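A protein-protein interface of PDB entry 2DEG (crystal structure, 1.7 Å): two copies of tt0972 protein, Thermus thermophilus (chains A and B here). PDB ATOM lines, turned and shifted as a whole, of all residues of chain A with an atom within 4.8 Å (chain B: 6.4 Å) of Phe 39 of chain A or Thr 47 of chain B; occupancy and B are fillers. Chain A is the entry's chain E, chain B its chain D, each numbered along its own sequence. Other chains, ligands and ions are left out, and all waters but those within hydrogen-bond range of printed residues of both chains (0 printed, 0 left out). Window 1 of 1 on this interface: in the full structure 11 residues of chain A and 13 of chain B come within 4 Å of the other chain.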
ATOM      1  N   ILE A  22     -13.866 -10.352  18.327  1.00  0.00           N
ATOM      2  CA  ILE A  22     -13.444  -9.081  18.957  1.00  0.00           C
ATOM      3  C   ILE A  22     -12.710  -9.388  20.264  1.00  0.00           C
ATOM      4  O   ILE A  22     -11.586  -8.919  20.469  1.00  0.00           O
ATOM      5  CB  ILE A  22     -14.641  -8.159  19.269  1.00  0.00           C
ATOM      6  CG1 ILE A  22     -15.242  -7.666  17.936  1.00  0.00           C
ATOM      7  CG2 ILE A  22     -14.228  -6.970  20.184  1.00  0.00           C
ATOM      8  CD1 ILE A  22     -16.626  -7.104  18.079  1.00  0.00           C
ATOM      9  N   LEU A  26      -8.734  -8.575  21.526  1.00  0.00           N
ATOM     10  CA  LEU A  26      -8.525  -7.771  22.753  1.00  0.00           C
ATOM     11  C   LEU A  26      -7.695  -8.563  23.757  1.00  0.00           C
ATOM     12  O   LEU A  26      -6.839  -7.997  24.458  1.00  0.00           O
ATOM     13  CB  LEU A  26      -9.834  -7.333  23.420  1.00  0.00           C
ATOM     14  CG  LEU A  26     -10.681  -6.300  22.632  1.00  0.00           C
ATOM     15  CD1 LEU A  26     -11.834  -5.750  23.462  1.00  0.00           C
ATOM     16  CD2 LEU A  26      -9.758  -5.191  22.063  1.00  0.00           C
ATOM     17  N   ASP A  37      -8.084   1.249  25.992  1.00  0.00           N
ATOM     18  CA  ASP A  37      -9.133   2.183  26.333  1.00  0.00           C
ATOM     19  C   ASP A  37     -10.397   1.868  25.501  1.00  0.00           C
ATOM     20  O   ASP A  37     -11.483   1.728  26.035  1.00  0.00           O
ATOM     21  CB  ASP A  37      -8.648   3.577  25.948  1.00  0.00           C
ATOM     22  CG  ASP A  37      -8.306   4.472  27.130  1.00  0.00           C
ATOM     23  OD1 ASP A  37      -9.237   5.168  27.602  1.00  0.00           O
ATOM     24  OD2 ASP A  37      -7.104   4.564  27.532  1.00  0.00           O
ATOM     25  N   TRP A  38     -10.235   1.767  24.188  1.00  0.00           N
ATOM     26  CA  TRP A  38     -11.434   1.665  23.296  1.00  0.00           C
ATOM     27  C   TRP A  38     -11.132   0.909  22.020  1.00  0.00           C
ATOM     28  O   TRP A  38      -9.986   0.763  21.649  1.00  0.00           O
ATOM     29  CB  TRP A  38     -11.968   3.067  22.944  1.00  0.00           C
ATOM     30  CG  TRP A  38     -11.317   3.738  21.745  1.00  0.00           C
ATOM     31  CD1 TRP A  38     -11.786   3.740  20.436  1.00  0.00           C
ATOM     32  CD2 TRP A  38     -10.137   4.542  21.735  1.00  0.00           C
ATOM     33  NE1 TRP A  38     -10.948   4.481  19.621  1.00  0.00           N
ATOM     34  CE2 TRP A  38      -9.926   4.981  20.389  1.00  0.00           C
ATOM     35  CE3 TRP A  38      -9.220   4.932  22.723  1.00  0.00           C
ATOM     36  CZ2 TRP A  38      -8.847   5.790  20.014  1.00  0.00           C
ATOM     37  CZ3 TRP A  38      -8.132   5.744  22.344  1.00  0.00           C
ATOM     38  CH2 TRP A  38      -7.951   6.157  20.994  1.00  0.00           C
ATOM     39  N   PHE A  39     -12.172   0.420  21.329  1.00  0.00           N
ATOM     40  CA  PHE A  39     -11.937  -0.169  20.023  1.00  0.00           C
ATOM     41  C   PHE A  39     -12.971   0.368  19.043  1.00  0.00           C
ATOM     42  O   PHE A  39     -14.034   0.836  19.445  1.00  0.00           O
ATOM     43  CB  PHE A  39     -11.999  -1.698  20.064  1.00  0.00           C
ATOM     44  CG  PHE A  39     -13.348  -2.244  20.471  1.00  0.00           C
ATOM     45  CD1 PHE A  39     -14.265  -2.590  19.508  1.00  0.00           C
ATOM     46  CD2 PHE A  39     -13.694  -2.427  21.817  1.00  0.00           C
ATOM     47  CE1 PHE A  39     -15.484  -3.108  19.834  1.00  0.00           C
ATOM     48  CE2 PHE A  39     -14.947  -2.927  22.173  1.00  0.00           C
ATOM     49  CZ  PHE A  39     -15.847  -3.270  21.180  1.00  0.00           C
ATOM     50  N   GLU A  40     -12.636   0.238  17.766  1.00  0.00           N
ATOM     51  CA  GLU A  40     -13.486   0.678  16.635  1.00  0.00           C
ATOM     52  C   GLU A  40     -13.474  -0.449  15.630  1.00  0.00           C
ATOM     53  O   GLU A  40     -12.426  -0.763  15.086  1.00  0.00           O
ATOM     54  CB  GLU A  40     -12.882   1.903  15.967  1.00  0.00           C
ATOM     55  CG  GLU A  40     -12.836   3.124  16.840  1.00  0.00           C
ATOM     56  CD  GLU A  40     -12.010   4.234  16.247  1.00  0.00           C
ATOM     57  OE1 GLU A  40     -11.794   4.255  15.005  1.00  0.00           O
ATOM     58  OE2 GLU A  40     -11.556   5.093  17.010  1.00  0.00           O
ATOM     59  N   VAL A  41     -14.653  -0.997  15.306  1.00  0.00           N
ATOM     60  CA  VAL A  41     -14.702  -2.046  14.269  1.00  0.00           C
ATOM     61  C   VAL A  41     -14.680  -1.430  12.884  1.00  0.00           C
ATOM     62  O   VAL A  41     -15.507  -0.549  12.580  1.00  0.00           O
ATOM     63  CB  VAL A  41     -15.941  -2.910  14.425  1.00  0.00           C
ATOM     64  CG1 VAL A  41     -16.047  -3.870  13.225  1.00  0.00           C
ATOM     65  CG2 VAL A  41     -15.901  -3.706  15.732  1.00  0.00           C
ATOM     66  N   LEU A  60     -10.349  -4.501  13.592  1.00  0.00           N
ATOM     67  CA  LEU A  60     -10.685  -3.412  14.500  1.00  0.00           C
ATOM     68  C   LEU A  60      -9.436  -2.602  14.825  1.00  0.00           C
ATOM     69  O   LEU A  60      -8.303  -3.086  14.687  1.00  0.00           O
ATOM     70  CB  LEU A  60     -11.416  -3.930  15.759  1.00  0.00           C
ATOM     71  CG  LEU A  60     -10.587  -4.904  16.625  1.00  0.00           C
ATOM     72  CD1 LEU A  60     -11.216  -5.067  17.999  1.00  0.00           C
ATOM     73  CD2 LEU A  60     -10.467  -6.264  15.975  1.00  0.00           C
ATOM     74  N   GLU A  61      -9.641  -1.352  15.210  1.00  0.00           N
ATOM     75  CA  GLU A  61      -8.567  -0.527  15.747  1.00  0.00           C
ATOM     76  C   GLU A  61      -8.667  -0.537  17.238  1.00  0.00           C
ATOM     77  O   GLU A  61      -9.753  -0.421  17.776  1.00  0.00           O
ATOM     78  CB  GLU A  61      -8.704   0.903  15.257  1.00  0.00           C
ATOM     79  CG  GLU A  61      -8.458   0.958  13.797  1.00  0.00           C
ATOM     80  CD  GLU A  61      -8.328   2.333  13.253  1.00  0.00           C
ATOM     81  OE1 GLU A  61      -9.305   3.103  13.363  1.00  0.00           O
ATOM     82  OE2 GLU A  61      -7.251   2.614  12.663  1.00  0.00           O
ATOM     83  N   VAL A  62      -7.534  -0.668  17.921  1.00  0.00           N
ATOM     84  CA  VAL A  62      -7.556  -0.687  19.383  1.00  0.00           C
ATOM     85  C   VAL A  62      -6.800   0.570  19.813  1.00  0.00           C
ATOM     86  O   VAL A  62      -5.690   0.764  19.354  1.00  0.00           O
ATOM     87  CB  VAL A  62      -6.880  -2.009  19.896  1.00  0.00           C
ATOM     88  CG1 VAL A  62      -6.595  -1.983  21.388  1.00  0.00           C
ATOM     89  CG2 VAL A  62      -7.739  -3.228  19.527  1.00  0.00           C
ATOM     90  N   ILE B  44     -19.618   0.468  14.837  1.00  0.00           N
ATOM     91  CA  ILE B  44     -19.632  -0.427  15.971  1.00  0.00           C
ATOM     92  C   ILE B  44     -18.310  -0.091  16.676  1.00  0.00           C
ATOM     93  O   ILE B  44     -17.255  -0.057  16.070  1.00  0.00           O
ATOM     94  CB  ILE B  44     -19.623  -1.896  15.506  1.00  0.00           C
ATOM     95  CG1 ILE B  44     -20.987  -2.262  14.876  1.00  0.00           C
ATOM     96  CG2 ILE B  44     -19.296  -2.803  16.687  1.00  0.00           C
ATOM     97  CD1 ILE B  44     -21.020  -3.653  14.245  1.00  0.00           C
ATOM     98  N   ARG B  45     -18.396   0.257  17.942  1.00  0.00           N
ATOM     99  CA  ARG B  45     -17.178   0.540  18.692  1.00  0.00           C
ATOM    100  C   ARG B  45     -17.359   0.053  20.089  1.00  0.00           C
ATOM    101  O   ARG B  45     -18.357  -0.567  20.398  1.00  0.00           O
ATOM    102  CB  ARG B  45     -16.827   2.027  18.644  1.00  0.00           C
ATOM    103  CG  ARG B  45     -17.886   3.021  19.042  1.00  0.00           C
ATOM    104  CD  ARG B  45     -17.578   4.386  18.379  1.00  0.00           C
ATOM    105  NE  ARG B  45     -16.304   4.967  18.832  1.00  0.00           N
ATOM    106  CZ  ARG B  45     -15.439   5.638  18.063  1.00  0.00           C
ATOM    107  NH1 ARG B  45     -15.691   5.840  16.773  1.00  0.00           N
ATOM    108  NH2 ARG B  45     -14.304   6.119  18.584  1.00  0.00           N
ATOM    109  N   GLY B  46     -16.410   0.310  20.964  1.00  0.00           N
ATOM    110  CA  GLY B  46     -16.711  -0.039  22.356  1.00  0.00           C
ATOM    111  C   GLY B  46     -15.580   0.394  23.271  1.00  0.00           C
ATOM    112  O   GLY B  46     -14.572   0.944  22.852  1.00  0.00           O
ATOM    113  N   THR B  47     -15.787   0.139  24.546  1.00  0.00           N
ATOM    114  CA  THR B  47     -14.750   0.393  25.541  1.00  0.00           C
ATOM    115  C   THR B  47     -14.145  -0.927  26.005  1.00  0.00           C
ATOM    116  O   THR B  47     -14.730  -2.017  25.847  1.00  0.00           O
ATOM    117  CB  THR B  47     -15.336   1.154  26.743  1.00  0.00           C
ATOM    118  OG1 THR B  47     -16.433   0.419  27.298  1.00  0.00           O
ATOM    119  CG2 THR B  47     -15.797   2.544  26.319  1.00  0.00           C
ATOM    120  N   ILE B  48     -12.968  -0.823  26.608  1.00  0.00           N
ATOM    121  CA  ILE B  48     -12.225  -2.007  27.006  1.00  0.00           C
ATOM    122  C   ILE B  48     -11.943  -1.948  28.492  1.00  0.00           C
ATOM    123  O   ILE B  48     -11.519  -0.904  28.994  1.00  0.00           O
ATOM    124  CB  ILE B  48     -10.881  -2.100  26.298  1.00  0.00           C
ATOM    125  CG1 ILE B  48     -11.036  -2.118  24.756  1.00  0.00           C
ATOM    126  CG2 ILE B  48     -10.142  -3.361  26.759  1.00  0.00           C
ATOM    127  CD1 ILE B  48      -9.758  -1.970  24.039  1.00  0.00           C
ATOM    128  N   GLY B  49     -12.188  -3.071  29.167  1.00  0.00           N
ATOM    129  CA  GLY B  49     -11.920  -3.226  30.615  1.00  0.00           C
ATOM    130  C   GLY B  49     -10.985  -4.398  30.853  1.00  0.00           C
ATOM    131  O   GLY B  49     -10.283  -4.871  29.957  1.00  0.00           O
ATOM    132  N   GLY B  52     -11.856  -7.659  28.753  1.00  0.00           N
ATOM    133  CA  GLY B  52     -12.008  -7.579  27.301  1.00  0.00           C
ATOM    134  C   GLY B  52     -12.987  -6.479  27.039  1.00  0.00           C
ATOM    135  O   GLY B  52     -12.838  -5.394  27.588  1.00  0.00           O
ATOM    136  N   VAL B  53     -14.040  -6.746  26.260  1.00  0.00           N
ATOM    137  CA  VAL B  53     -15.005  -5.673  26.034  1.00  0.00           C
ATOM    138  C   VAL B  53     -15.671  -5.313  27.335  1.00  0.00           C
ATOM    139  O   VAL B  53     -16.135  -6.196  28.065  1.00  0.00           O
ATOM    140  CB  VAL B  53     -16.119  -6.099  25.047  1.00  0.00           C
ATOM    141  CG1 VAL B  53     -17.055  -4.939  24.780  1.00  0.00           C
ATOM    142  CG2 VAL B  53     -15.499  -6.573  23.747  1.00  0.00           C
ATOM    143  N   LYS B  54     -15.747  -4.015  27.620  1.00  0.00           N
ATOM    144  CA  LYS B  54     -16.525  -3.512  28.724  1.00  0.00           C
ATOM    145  C   LYS B  54     -17.949  -3.224  28.245  1.00  0.00           C
ATOM    146  O   LYS B  54     -18.891  -3.920  28.634  1.00  0.00           O
ATOM    147  CB  LYS B  54     -15.860  -2.246  29.251  1.00  0.00           C
ATOM    148  CG  LYS B  54     -16.478  -1.691  30.499  1.00  0.00           C
ATOM    149  CD  LYS B  54     -15.834  -0.347  30.842  1.00  0.00           C
ATOM    150  CE  LYS B  54     -14.332  -0.445  30.988  1.00  0.00           C
ATOM    151  NZ  LYS B  54     -13.749   0.878  31.254  1.00  0.00           N
ATOM    152  N   GLU B  55     -18.114  -2.231  27.368  1.00  0.00           N
ATOM    153  CA  GLU B  55     -19.430  -2.053  26.733  1.00  0.00           C
ATOM    154  C   GLU B  55     -19.283  -2.026  25.226  1.00  0.00           C
ATOM    155  O   GLU B  55     -18.327  -1.477  24.705  1.00  0.00           O
ATOM    156  CB  GLU B  55     -20.071  -0.740  27.155  1.00  0.00           C
ATOM    157  CG  GLU B  55     -20.722  -0.805  28.510  1.00  0.00           C
ATOM    158  CD  GLU B  55     -21.406   0.483  28.875  1.00  0.00           C
ATOM    159  OE1 GLU B  55     -20.944   1.572  28.440  1.00  0.00           O
ATOM    160  OE2 GLU B  55     -22.427   0.382  29.596  1.00  0.00           O
ATOM    161  N   TYR B  56     -20.251  -2.614  24.539  1.00  0.00           N
ATOM    162  CA  TYR B  56     -20.363  -2.448  23.097  1.00  0.00           C
ATOM    163  C   TYR B  56     -21.162  -1.204  22.879  1.00  0.00           C
ATOM    164  O   TYR B  56     -22.128  -0.971  23.585  1.00  0.00           O
ATOM    165  CB  TYR B  56     -21.141  -3.623  22.483  1.00  0.00           C
ATOM    166  CG  TYR B  56     -20.387  -4.915  22.577  1.00  0.00           C
ATOM    167  CD1 TYR B  56     -19.415  -5.224  21.636  1.00  0.00           C
ATOM    168  CD2 TYR B  56     -20.666  -5.836  23.598  1.00  0.00           C
ATOM    169  CE1 TYR B  56     -18.707  -6.424  21.694  1.00  0.00           C
ATOM    170  CE2 TYR B  56     -19.954  -7.047  23.669  1.00  0.00           C
ATOM    171  CZ  TYR B  56     -19.009  -7.323  22.705  1.00  0.00           C
ATOM    172  OH  TYR B  56     -18.270  -8.483  22.758  1.00  0.00           O
ATOM    173  N   GLN B  57     -20.784  -0.422  21.857  1.00  0.00           N
ATOM    174  CA  GLN B  57     -21.544   0.760  21.540  1.00  0.00           C
ATOM    175  C   GLN B  57     -21.880   0.736  20.055  1.00  0.00           C
ATOM    176  O   GLN B  57     -20.969   0.691  19.210  1.00  0.00           O
ATOM    177  CB  GLN B  57     -20.703   1.981  21.810  1.00  0.00           C
ATOM    178  CG  GLN B  57     -20.254   2.017  23.276  1.00  0.00           C
ATOM    179  CD  GLN B  57     -19.122   2.959  23.521  1.00  0.00           C
ATOM    180  OE1 GLN B  57     -18.302   3.227  22.651  1.00  0.00           O
ATOM    181  NE2 GLN B  57     -19.079   3.494  24.737  1.00  0.00           N
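Of the 12 printed residues of chain B, 7 touch a printed residue of chain A.
Hydrophobic or aromatic side chains of chain B within 4 Å of the printed part of chain A: Ile 44, Ile 48 and Val 53.
Hydrophobic or aromatic side chains of chain A that line the printed part of chain B: Ile 22, Leu 26, Trp 38, Phe 39 and Val 41.
Among the printed residues, 17 pairs touch across the chains.
Among the printed residues, Asp or Glu carboxylates within 4 Å of a Lys or Arg side-chain nitrogen of the other chain: Glu 40 of chain A with Arg 45 of chain B (3.3 Å).
Of the printed residues of chain B, Leu 26 of chain A touches Ile 48, Gly 52 and Val 53.
Phe 39 of chain A touches just these residues of chain B: Arg 45, Gly 46, Thr 47, Ile 48 and Val 53.
Printed residues of chain A within 4 Å of Ile 44 of chain B: Glu 40 (3.8 Å) and Val 41 (2.9 Å).
Printed residues of chain A within 4 Å of Arg 45 of chain B: Trp 38 (3.9 Å), Phe 39 (3.1 Å) and Glu 40 (3.3 Å).
Thr 47 of chain B touches just these residues of chain A: Asp 37 and Phe 39.
Printed residues of chain A within 4 Å of Ile 48 of chain B: Leu 26, Asp 37, Trp 38 and Phe 39.
Gly 49 of chain B touches none of the printed residues of chain A.
The nearest residue of chain B that does not touch Phe 39 of chain A is Tyr 56 of chain B (4.1 Å).
The nearest printed residue of chain A that does not touch Arg 45 of chain B is Val 41 of chain A (4.5 Å).
The backbone NH (N) of Val 41 of chain A is in hydrogen-bond range of the backbone carbonyl oxygen (O) of Ile 44 of chain B (2.9 Å).
NH2 of Arg 45 of chain B lies within salt-bridge range of OE2 of Glu 40 of chain A.
The backbone carbonyl oxygen (O) of Phe 39 of chain A sits at hydrogen-bond distance from the backbone NH (N) of Gly 46 of chain B.
The backbone NH of Ile 48 of chain B lies within hydrogen-bond range of the backbone carbonyl oxygen of Asp 37 of chain A (3.0 Å).
O of Arg 45 of chain B sits at hydrogen-bond distance from N of Gln 57 of chain B, at 2.8 Å.
The backbone NH (N) of Lys 54 of chain B is in hydrogen-bond range of the backbone carbonyl oxygen (O) of Thr 47 of chain B, at 2.9 Å.
O of Glu 55 of chain B lies within hydrogen-bond range of N of Thr 47 of chain B.
NE1 of Trp 38 of chain A sits at hydrogen-bond distance from OE2 of Glu 40 of chain A (2.7 Å).
The backbone carbonyl oxygen (O) of Glu 40 of chain A is in hydrogen-bond range of the backbone NH (N) of Glu 61 of chain A (2.8 Å).
No position is printed for both chains.
Of the 17 pairs that touch across the chains among the printed residues, none has its exchanged pair printed and touching as well.
Ile 22 of chain A touches Val 53 of chain B.
CD2 of Leu 26 of chain A touches CD1 of Ile 48 of chain B, 3.8 Å away.
Leu 26 of chain A touches Gly 52 of chain B (CD1 to C, 3.8 Å).
O of Asp 37 of chain A touches CA of Thr 47 of chain B (3.6 Å).
Trp 38 of chain A touches Arg 45 of chain B.
Gly 46 of chain B touches Trp 38 of chain A.
Ile 48 of chain B touches Trp 38 of chain A (CD1 to O, 3.6 Å).
Phe 39 of chain A touches Arg 45 of chain B (O to CB, 3.1 Å).
Thr 47 of chain B touches Phe 39 of chain A.
Phe 39 of chain A touches Ile 48 of chain B (CD2 to CG1, 3.97 Å).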
